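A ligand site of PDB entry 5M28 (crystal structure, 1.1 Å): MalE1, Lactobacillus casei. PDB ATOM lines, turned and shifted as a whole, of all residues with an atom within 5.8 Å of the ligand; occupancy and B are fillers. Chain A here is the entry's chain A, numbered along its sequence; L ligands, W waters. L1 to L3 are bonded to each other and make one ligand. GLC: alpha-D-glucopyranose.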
ATOM      1  N   ASP A  12      -1.293  -5.613 -27.113  1.00  0.00           N
ATOM      2  CA  ASP A  12      -0.894  -5.935 -25.744  1.00  0.00           C
ATOM      3  C   ASP A  12      -2.126  -6.257 -24.897  1.00  0.00           C
ATOM      4  O   ASP A  12      -3.252  -5.853 -25.185  1.00  0.00           O
ATOM      5  CB  ASP A  12      -0.081  -4.773 -25.154  1.00  0.00           C
ATOM      6  CG  ASP A  12       1.288  -4.624 -25.809  1.00  0.00           C
ATOM      7  OD1 ASP A  12       1.838  -5.647 -26.249  1.00  0.00           O
ATOM      8  OD2 ASP A  12       1.826  -3.507 -25.915  1.00  0.00           O
ATOM      9  N   THR A  13      -1.895  -6.995 -23.807  1.00  0.00           N
ATOM     10  CA  THR A  13      -2.982  -7.641 -23.056  1.00  0.00           C
ATOM     11  C   THR A  13      -4.173  -6.728 -22.721  1.00  0.00           C
ATOM     12  O   THR A  13      -5.333  -7.042 -23.006  1.00  0.00           O
ATOM     13  CB  THR A  13      -2.374  -8.275 -21.814  1.00  0.00           C
ATOM     14  OG1 THR A  13      -1.358  -9.200 -22.232  1.00  0.00           O
ATOM     15  CG2 THR A  13      -3.428  -9.012 -20.999  1.00  0.00           C
ATOM     16  N   GLN A  15      -5.054  -3.980 -23.902  1.00  0.00           N
ATOM     17  CA  GLN A  15      -5.550  -3.211 -25.043  1.00  0.00           C
ATOM     18  C   GLN A  15      -6.626  -3.956 -25.820  1.00  0.00           C
ATOM     19  O   GLN A  15      -7.334  -3.335 -26.617  1.00  0.00           O
ATOM     20  CB  GLN A  15      -4.402  -2.895 -25.993  1.00  0.00           C
ATOM     21  CG  GLN A  15      -3.260  -2.107 -25.369  1.00  0.00           C
ATOM     22  CD  GLN A  15      -2.120  -1.857 -26.343  1.00  0.00           C
ATOM     23  OE1 GLN A  15      -1.416  -0.847 -26.262  1.00  0.00           O
ATOM     24  NE2 GLN A  15      -1.939  -2.734 -27.259  1.00  0.00           N
ATOM     25  N   GLY A  43       4.121  -9.594 -25.872  1.00  0.00           N
ATOM     26  CA  GLY A  43       4.002  -8.147 -25.841  1.00  0.00           C
ATOM     27  C   GLY A  43       4.768  -7.465 -26.960  1.00  0.00           C
ATOM     28  O   GLY A  43       5.707  -8.004 -27.551  1.00  0.00           O
ATOM     29  N   SER A  44       4.361  -6.218 -27.234  1.00  0.00           N
ATOM     30  CA  SER A  44       4.981  -5.389 -28.254  1.00  0.00           C
ATOM     31  C   SER A  44       6.455  -5.145 -27.999  1.00  0.00           C
ATOM     32  O   SER A  44       7.219  -4.974 -28.967  1.00  0.00           O
ATOM     33  CB  SER A  44       4.239  -4.047 -28.312  1.00  0.00           C
ATOM     34  OG  SER A  44       4.248  -3.391 -27.048  1.00  0.00           O
ATOM     35  N   ALA A  45       6.893  -5.126 -26.735  1.00  0.00           N
ATOM     36  CA  ALA A  45       8.298  -4.969 -26.433  1.00  0.00           C
ATOM     37  C   ALA A  45       9.113  -6.169 -26.879  1.00  0.00           C
ATOM     38  O   ALA A  45      10.341  -6.104 -26.862  1.00  0.00           O
ATOM     39  CB  ALA A  45       8.498  -4.722 -24.944  1.00  0.00           C
ATOM     40  N   ASN A  46       8.449  -7.260 -27.276  1.00  0.00           N
ATOM     41  CA  ASN A  46       9.091  -8.510 -27.705  1.00  0.00           C
ATOM     42  C   ASN A  46       8.585  -8.963 -29.070  1.00  0.00           C
ATOM     43  O   ASN A  46       8.709 -10.142 -29.409  1.00  0.00           O
ATOM     44  CB  ASN A  46       8.859  -9.590 -26.654  1.00  0.00           C
ATOM     45  CG  ASN A  46       9.511  -9.250 -25.345  1.00  0.00           C
ATOM     46  OD1 ASN A  46      10.734  -9.120 -25.278  1.00  0.00           O
ATOM     47  ND2 ASN A  46       8.723  -9.107 -24.304  1.00  0.00           N
ATOM     48  N   LYS A  48       9.937  -8.506 -31.918  1.00  0.00           N
ATOM     49  CA  LYS A  48      11.143  -8.993 -32.592  1.00  0.00           C
ATOM     50  C   LYS A  48      11.251 -10.507 -32.515  1.00  0.00           C
ATOM     51  O   LYS A  48      11.482 -11.195 -33.512  1.00  0.00           O
ATOM     52  CB  LYS A  48      12.420  -8.325 -31.969  1.00  0.00           C
ATOM     53  CG  LYS A  48      12.482  -8.125 -30.399  1.00  0.00           C
ATOM     54  CD  LYS A  48      13.711  -7.297 -29.873  1.00  0.00           C
ATOM     55  CE  LYS A  48      13.510  -6.784 -28.428  1.00  0.00           C
ATOM     56  NZ  LYS A  48      14.602  -5.861 -27.929  1.00  0.00           N
ATOM     57  N   GLU A  63       1.650  -5.166 -33.027  1.00  0.00           N
ATOM     58  CA  GLU A  63       2.162  -3.986 -32.359  1.00  0.00           C
ATOM     59  C   GLU A  63       3.658  -4.141 -32.098  1.00  0.00           C
ATOM     60  O   GLU A  63       4.117  -5.208 -31.668  1.00  0.00           O
ATOM     61  CB  GLU A  63       1.398  -3.789 -31.052  1.00  0.00           C
ATOM     62  CG  GLU A  63       1.594  -2.413 -30.431  1.00  0.00           C
ATOM     63  CD  GLU A  63       0.676  -2.161 -29.263  1.00  0.00           C
ATOM     64  OE1 GLU A  63      -0.303  -2.933 -29.136  1.00  0.00           O
ATOM     65  OE2 GLU A  63       0.868  -1.200 -28.502  1.00  0.00           O
ATOM     66  N   ALA A  65       7.353  -1.640 -31.063  1.00  0.00           N
ATOM     67  CA  ALA A  65       8.032  -0.375 -30.803  1.00  0.00           C
ATOM     68  C   ALA A  65       9.083  -0.091 -31.878  1.00  0.00           C
ATOM     69  O   ALA A  65       9.671  -1.004 -32.458  1.00  0.00           O
ATOM     70  CB  ALA A  65       8.700  -0.412 -29.428  1.00  0.00           C
ATOM     71  N   ASN A  66       9.361   1.193 -32.103  1.00  0.00           N
ATOM     72  CA  ASN A  66      10.118   1.570 -33.302  1.00  0.00           C
ATOM     73  C   ASN A  66      11.552   1.067 -33.299  1.00  0.00           C
ATOM     74  O   ASN A  66      12.141   0.908 -34.372  1.00  0.00           O
ATOM     75  CB  ASN A  66      10.095   3.086 -33.495  1.00  0.00           C
ATOM     76  CG  ASN A  66      11.014   3.822 -32.534  1.00  0.00           C
ATOM     77  OD1 ASN A  66      10.683   4.026 -31.368  1.00  0.00           O
ATOM     78  ND2 ASN A  66      12.164   4.250 -33.044  1.00  0.00           N
ATOM     79  N   ASP A  67      12.143   0.822 -32.131  1.00  0.00           N
ATOM     80  CA  ASP A  67      13.536   0.383 -32.087  1.00  0.00           C
ATOM     81  C   ASP A  67      13.746  -0.965 -32.757  1.00  0.00           C
ATOM     82  O   ASP A  67      14.877  -1.264 -33.164  1.00  0.00           O
ATOM     83  CB  ASP A  67      14.051   0.305 -30.646  1.00  0.00           C
ATOM     84  CG  ASP A  67      13.320  -0.730 -29.810  1.00  0.00           C
ATOM     85  OD1 ASP A  67      12.088  -0.555 -29.648  1.00  0.00           O
ATOM     86  OD2 ASP A  67      13.964  -1.681 -29.309  1.00  0.00           O
ATOM     87  N   GLN A  68      12.704  -1.789 -32.859  1.00  0.00           N
ATOM     88  CA  GLN A  68      12.835  -3.132 -33.402  1.00  0.00           C
ATOM     89  C   GLN A  68      12.792  -3.158 -34.926  1.00  0.00           C
ATOM     90  O   GLN A  68      13.014  -4.219 -35.531  1.00  0.00           O
ATOM     91  CB  GLN A  68      11.730  -4.014 -32.832  1.00  0.00           C
ATOM     92  CG  GLN A  68      11.868  -4.170 -31.330  1.00  0.00           C
ATOM     93  CD  GLN A  68      10.720  -4.875 -30.714  1.00  0.00           C
ATOM     94  OE1 GLN A  68      10.189  -5.843 -31.259  1.00  0.00           O
ATOM     95  NE2 GLN A  68      10.221  -4.316 -29.609  1.00  0.00           N
ATOM     96  N   GLN A 115       5.668   7.990 -27.132  1.00  0.00           N
ATOM     97  CA  GLN A 115       5.956   7.489 -25.788  1.00  0.00           C
ATOM     98  C   GLN A 115       7.201   8.140 -25.212  1.00  0.00           C
ATOM     99  O   GLN A 115       8.298   7.985 -25.757  1.00  0.00           O
ATOM    100  CB  GLN A 115       6.134   5.977 -25.812  1.00  0.00           C
ATOM    101  CG  GLN A 115       4.892   5.238 -26.236  1.00  0.00           C
ATOM    102  CD  GLN A 115       5.045   3.733 -26.271  1.00  0.00           C
ATOM    103  OE1 GLN A 115       6.169   3.202 -26.273  1.00  0.00           O
ATOM    104  NE2 GLN A 115       3.923   3.024 -26.284  1.00  0.00           N
ATOM    105  N   GLN A 117       8.698   8.485 -21.080  1.00  0.00           N
ATOM    106  CA  GLN A 117       8.434   8.394 -19.661  1.00  0.00           C
ATOM    107  C   GLN A 117       8.483   9.764 -19.001  1.00  0.00           C
ATOM    108  O   GLN A 117       9.128  10.713 -19.468  1.00  0.00           O
ATOM    109  CB  GLN A 117       9.393   7.421 -18.982  1.00  0.00           C
ATOM    110  CG  GLN A 117       9.161   6.000 -19.481  1.00  0.00           C
ATOM    111  CD  GLN A 117       9.681   4.876 -18.597  1.00  0.00           C
ATOM    112  OE1 GLN A 117       9.236   3.741 -18.745  1.00  0.00           O
ATOM    113  NE2 GLN A 117      10.631   5.155 -17.724  1.00  0.00           N
ATOM    114  N   ASN A 149      16.150  -2.524 -15.843  1.00  0.00           N
ATOM    115  CA  ASN A 149      15.460  -2.175 -17.081  1.00  0.00           C
ATOM    116  C   ASN A 149      16.238  -1.044 -17.747  1.00  0.00           C
ATOM    117  O   ASN A 149      16.221   0.093 -17.283  1.00  0.00           O
ATOM    118  CB  ASN A 149      14.020  -1.783 -16.782  1.00  0.00           C
ATOM    119  CG  ASN A 149      13.225  -1.502 -18.043  1.00  0.00           C
ATOM    120  OD1 ASN A 149      13.799  -1.177 -19.081  1.00  0.00           O
ATOM    121  ND2 ASN A 149      11.909  -1.616 -17.965  1.00  0.00           N
ATOM    122  N   ALA A 150      16.968  -1.377 -18.814  1.00  0.00           N
ATOM    123  CA  ALA A 150      17.826  -0.406 -19.493  1.00  0.00           C
ATOM    124  C   ALA A 150      17.026   0.701 -20.173  1.00  0.00           C
ATOM    125  O   ALA A 150      17.575   1.780 -20.434  1.00  0.00           O
ATOM    126  CB  ALA A 150      18.716  -1.100 -20.518  1.00  0.00           C
ATOM    127  N   TYR A 151      15.761   0.457 -20.502  1.00  0.00           N
ATOM    128  CA  TYR A 151      14.924   1.516 -21.039  1.00  0.00           C
ATOM    129  C   TYR A 151      14.729   2.627 -20.019  1.00  0.00           C
ATOM    130  O   TYR A 151      14.595   3.794 -20.398  1.00  0.00           O
ATOM    131  CB  TYR A 151      13.595   0.913 -21.487  1.00  0.00           C
ATOM    132  CG  TYR A 151      12.579   1.880 -22.059  1.00  0.00           C
ATOM    133  CD1 TYR A 151      12.592   2.217 -23.407  1.00  0.00           C
ATOM    134  CD2 TYR A 151      11.592   2.414 -21.256  1.00  0.00           C
ATOM    135  CE1 TYR A 151      11.608   3.056 -23.935  1.00  0.00           C
ATOM    136  CE2 TYR A 151      10.598   3.233 -21.774  1.00  0.00           C
ATOM    137  CZ  TYR A 151      10.612   3.558 -23.114  1.00  0.00           C
ATOM    138  OH  TYR A 151       9.631   4.374 -23.626  1.00  0.00           O
ATOM    139  N   TRP A 221       1.523   4.375 -21.577  1.00  0.00           N
ATOM    140  CA  TRP A 221       0.734   3.140 -21.573  1.00  0.00           C
ATOM    141  C   TRP A 221       0.095   2.908 -20.207  1.00  0.00           C
ATOM    142  O   TRP A 221      -0.911   2.188 -20.111  1.00  0.00           O
ATOM    143  CB  TRP A 221       1.595   1.940 -22.013  1.00  0.00           C
ATOM    144  CG  TRP A 221       2.863   1.806 -21.232  1.00  0.00           C
ATOM    145  CD1 TRP A 221       3.029   1.141 -20.058  1.00  0.00           C
ATOM    146  CD2 TRP A 221       4.131   2.402 -21.526  1.00  0.00           C
ATOM    147  NE1 TRP A 221       4.322   1.267 -19.615  1.00  0.00           N
ATOM    148  CE2 TRP A 221       5.015   2.056 -20.486  1.00  0.00           C
ATOM    149  CE3 TRP A 221       4.608   3.174 -22.586  1.00  0.00           C
ATOM    150  CZ2 TRP A 221       6.342   2.464 -20.476  1.00  0.00           C
ATOM    151  CZ3 TRP A 221       5.924   3.574 -22.574  1.00  0.00           C
ATOM    152  CH2 TRP A 221       6.778   3.222 -21.525  1.00  0.00           C
ATOM    153  N   GLU A 258       5.290   4.031 -30.885  1.00  0.00           N
ATOM    154  CA  GLU A 258       4.607   2.745 -30.953  1.00  0.00           C
ATOM    155  C   GLU A 258       3.935   2.646 -32.316  1.00  0.00           C
ATOM    156  O   GLU A 258       3.379   3.621 -32.821  1.00  0.00           O
ATOM    157  CB  GLU A 258       3.565   2.598 -29.848  1.00  0.00           C
ATOM    158  CG  GLU A 258       3.173   1.154 -29.578  1.00  0.00           C
ATOM    159  CD  GLU A 258       4.327   0.368 -29.022  1.00  0.00           C
ATOM    160  OE1 GLU A 258       5.069   0.894 -28.190  1.00  0.00           O
ATOM    161  OE2 GLU A 258       4.538  -0.770 -29.403  1.00  0.00           O
ATOM    162  N   GLN A 296      -2.614   6.968 -23.820  1.00  0.00           N
ATOM    163  CA  GLN A 296      -1.466   7.107 -24.704  1.00  0.00           C
ATOM    164  C   GLN A 296      -1.656   8.305 -25.632  1.00  0.00           C
ATOM    165  O   GLN A 296      -2.770   8.688 -25.994  1.00  0.00           O
ATOM    166  CB  GLN A 296      -1.185   5.837 -25.499  1.00  0.00           C
ATOM    167  CG  GLN A 296      -0.632   4.716 -24.670  1.00  0.00           C
ATOM    168  CD  GLN A 296       0.402   3.910 -25.392  1.00  0.00           C
ATOM    169  OE1 GLN A 296       1.419   4.448 -25.840  1.00  0.00           O
ATOM    170  NE2 GLN A 296       0.180   2.596 -25.488  1.00  0.00           N
ATOM    171  N   MET A 330      14.567   6.511 -29.729  1.00  0.00           N
ATOM    172  CA  MET A 330      15.225   5.214 -29.708  1.00  0.00           C
ATOM    173  C   MET A 330      15.778   4.898 -31.099  1.00  0.00           C
ATOM    174  O   MET A 330      14.990   4.881 -32.065  1.00  0.00           O
ATOM    175  CB  MET A 330      14.289   4.065 -29.359  1.00  0.00           C
ATOM    176  CG  MET A 330      13.828   4.064 -27.924  1.00  0.00           C
ATOM    177  SD  MET A 330      13.060   2.485 -27.434  1.00  0.00           S
ATOM    178  CE  MET A 330      11.515   2.520 -28.337  1.00  0.00           C
ATOM    179  N   TRP A 340      20.210  -3.825 -25.974  1.00  0.00           N
ATOM    180  CA  TRP A 340      19.392  -3.890 -24.765  1.00  0.00           C
ATOM    181  C   TRP A 340      19.885  -4.994 -23.845  1.00  0.00           C
ATOM    182  O   TRP A 340      19.895  -4.828 -22.624  1.00  0.00           O
ATOM    183  CB  TRP A 340      17.925  -4.141 -25.112  1.00  0.00           C
ATOM    184  CG  TRP A 340      17.235  -3.038 -25.843  1.00  0.00           C
ATOM    185  CD1 TRP A 340      16.706  -3.112 -27.098  1.00  0.00           C
ATOM    186  CD2 TRP A 340      16.958  -1.717 -25.362  1.00  0.00           C
ATOM    187  NE1 TRP A 340      16.144  -1.913 -27.449  1.00  0.00           N
ATOM    188  CE2 TRP A 340      16.264  -1.049 -26.392  1.00  0.00           C
ATOM    189  CE3 TRP A 340      17.228  -1.032 -24.162  1.00  0.00           C
ATOM    190  CZ2 TRP A 340      15.834   0.267 -26.250  1.00  0.00           C
ATOM    191  CZ3 TRP A 340      16.789   0.280 -24.040  1.00  0.00           C
ATOM    192  CH2 TRP A 340      16.109   0.903 -25.074  1.00  0.00           C
HETATM  193  C1  GLC L   1       2.790  -2.967 -22.168  1.00  0.00           C
HETATM  194  C2  GLC L   1       2.667  -1.688 -22.981  1.00  0.00           C
HETATM  195  C3  GLC L   1       3.991  -1.380 -23.668  1.00  0.00           C
HETATM  196  C4  GLC L   1       5.090  -1.307 -22.615  1.00  0.00           C
HETATM  197  C5  GLC L   1       5.135  -2.583 -21.784  1.00  0.00           C
HETATM  198  C6  GLC L   1       6.113  -2.480 -20.637  1.00  0.00           C
HETATM  199  O1  GLC L   1       3.003  -4.049 -23.014  1.00  0.00           O
HETATM  200  O2  GLC L   1       1.594  -1.756 -23.912  1.00  0.00           O
HETATM  201  O3  GLC L   1       3.862  -0.145 -24.337  1.00  0.00           O
HETATM  202  O4  GLC L   1       6.345  -1.142 -23.290  1.00  0.00           O
HETATM  203  O5  GLC L   1       3.830  -2.813 -21.215  1.00  0.00           O
HETATM  204  O6  GLC L   1       6.238  -3.713 -19.977  1.00  0.00           O
HETATM  205  C1  GLC L   2       7.041   0.050 -23.043  1.00  0.00           C
HETATM  206  C2  GLC L   2       7.501   0.653 -24.366  1.00  0.00           C
HETATM  207  C3  GLC L   2       8.626  -0.157 -24.991  1.00  0.00           C
HETATM  208  C4  GLC L   2       9.734  -0.440 -23.982  1.00  0.00           C
HETATM  209  C5  GLC L   2       9.181  -1.019 -22.686  1.00  0.00           C
HETATM  210  C6  GLC L   2      10.252  -1.108 -21.618  1.00  0.00           C
HETATM  211  O2  GLC L   2       6.388   0.698 -25.245  1.00  0.00           O
HETATM  212  O3  GLC L   2       9.159   0.579 -26.089  1.00  0.00           O
HETATM  213  O4  GLC L   2      10.620  -1.417 -24.551  1.00  0.00           O
HETATM  214  O5  GLC L   2       8.149  -0.147 -22.177  1.00  0.00           O
HETATM  215  O6  GLC L   2       9.815  -1.775 -20.438  1.00  0.00           O
HETATM  216  C1  GLC L   3      11.874  -0.948 -25.002  1.00  0.00           C
HETATM  217  C2  GLC L   3      12.134  -1.448 -26.410  1.00  0.00           C
HETATM  218  C3  GLC L   3      12.325  -2.964 -26.428  1.00  0.00           C
HETATM  219  C4  GLC L   3      13.440  -3.314 -25.460  1.00  0.00           C
HETATM  220  C5  GLC L   3      13.099  -2.794 -24.072  1.00  0.00           C
HETATM  221  C6  GLC L   3      14.214  -3.033 -23.088  1.00  0.00           C
HETATM  222  O2  GLC L   3      11.050  -1.046 -27.235  1.00  0.00           O
HETATM  223  O3  GLC L   3      12.625  -3.448 -27.738  1.00  0.00           O
HETATM  224  O4  GLC L   3      13.602  -4.742 -25.414  1.00  0.00           O
HETATM  225  O5  GLC L   3      12.911  -1.359 -24.129  1.00  0.00           O
HETATM  226  O6  GLC L   3      13.818  -2.740 -21.758  1.00  0.00           O
HETATM  227  O   HOH W   1      -0.830  -1.975 -22.717  1.00  0.00           O
HETATM  228  O   HOH W   2      16.063  -3.708 -20.218  1.00  0.00           O
HETATM  229  O   HOH W   3       8.401  -0.570 -18.355  1.00  0.00           O
HETATM  230  O   HOH W   4       6.211  -1.543 -27.091  1.00  0.00           O
HETATM  231  O   HOH W   5       8.917   3.420 -26.072  1.00  0.00           O
HETATM  232  O   HOH W   6       5.247  -5.403 -24.295  1.00  0.00           O
HETATM  233  O   HOH W   7       7.027  -5.852 -21.824  1.00  0.00           O
HETATM  234  O   HOH W   8       2.007   0.490 -26.400  1.00  0.00           O
HETATM  235  O   HOH W   9       1.883  -6.098 -21.697  1.00  0.00           O
HETATM  236  O   HOH W  10      11.906  -6.442 -24.484  1.00  0.00           O
HETATM  237  O   HOH W  11       7.886  -3.354 -17.722  1.00  0.00           O
HETATM  238  O   HOH W  12      11.772  -3.951 -20.597  1.00  0.00           O
HETATM  239  O   HOH W  13       9.282  -4.588 -21.208  1.00  0.00           O
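Water W10 lies within hydrogen-bond range of O4 of GLC L3 (2.6 Å), O of Ala 45 (2.9 Å) and OD1 of Asn 46 (3.0 Å).
Water W8 lies within hydrogen-bond range of an oxygen (O3) of GLC L1 (2.8 Å), the side-chain carboxylate of Glu 63 (2.9 Å), the side-chain amide nitrogen of Gln 296 (2.9 Å) and the side-chain amide nitrogen of Gln 115 (3.2 Å).
Water W5 lies within hydrogen-bond range of OH of Tyr 151 (2.7 Å), OE1 of Gln 115 (2.8 Å) and O3 of GLC L2 (2.9 Å).
Water W2 bridges the backbone NH (N) of Ala 150 (2.9 Å) and an oxygen (O6) of GLC L3 (2.9 Å).
Water W4 lies within hydrogen-bond range of the side-chain hydroxyl of Ser 44, the side-chain carboxylate of Glu 258 and an oxygen (O2) of GLC L2.
Water W6 lies within hydrogen-bond range of an oxygen (O1) of GLC L1 (2.9 Å), the backbone NH of Ala 45 (3.0 Å) and the backbone NH of Ser 44 (3.2 Å).
NZ of Lys 48 lies within hydrogen-bond range of O4 of GLC L3, 2.9 Å away.
O2 of GLC L1 is in hydrogen-bond range of OD2 of Asp 12, at 2.7 Å.
The side-chain amide oxygen of Gln 115 sits at hydrogen-bond distance from an oxygen (O2) of GLC L2 (2.7 Å).
The side-chain amide nitrogen (NE2) of Gln 68 sits at hydrogen-bond distance from an oxygen (O3) of GLC L3, 3.2 Å away.
O2 of GLC L2 is in hydrogen-bond range of OE1 of Glu 258 (3.2 Å).
OD1 of Asn 149 is in hydrogen-bond range of O6 of GLC L3 (3.1 Å).
OD1 of Asp 67 sits at hydrogen-bond distance from O2 of GLC L3, at 2.7 Å.
OE1 of Gln 15 touches O2 of GLC L1, at 3.9 Å.
OG of Ser 44 touches C3 of GLC L1, at 3.9 Å.
O of Ala 45 touches O3 of GLC L3 (3.6 Å).
CB of Ala 65 touches O2 of GLC L3, at 3.3 Å.
CB of Tyr 151 touches O5 of GLC L3, 3.6 Å away.
Trp 221 touches the ligand.
CE of Met 330 touches O2 of GLC L3, 3.8 Å away.
NE1 of Trp 340 touches C4 of GLC L3 (3.6 Å).
Hydrophobic or aromatic side chains that line the ligand: Ala 45, Ala 65, Tyr 151, Trp 221, Met 330 and Trp 340.
Of the 23 residues printed, 15 come within 4 Å of the ligand.
The side-chain amide nitrogen (NE2) of Gln 115 is in hydrogen-bond range of the side-chain carboxylate (OE1) of Glu 258, at 3.1 Å.
OD2 of Asp 67 is in hydrogen-bond range of NE1 of Trp 340, 2.9 Å away.
The backbone NH of Asp 12 lies close to the side-chain amide nitrogen of Gln 15 (3.0 Å).
O of Ala 45 sits at hydrogen-bond distance from NE2 of Gln 68 (3.3 Å).
OE1 of Gln 296 sits at hydrogen-bond distance from NE2 of Gln 115 (2.9 Å).
The side-chain amide nitrogen of Gln 15 is in hydrogen-bond range of the side-chain carboxylate of Glu 63 (2.5 Å).
The backbone NH of Lys 48 is in hydrogen-bond range of the side-chain amide oxygen of Gln 68.
The backbone carbonyl oxygen (O) of Met 330 sits at hydrogen-bond distance from the side-chain amide nitrogen (ND2) of Asn 66.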
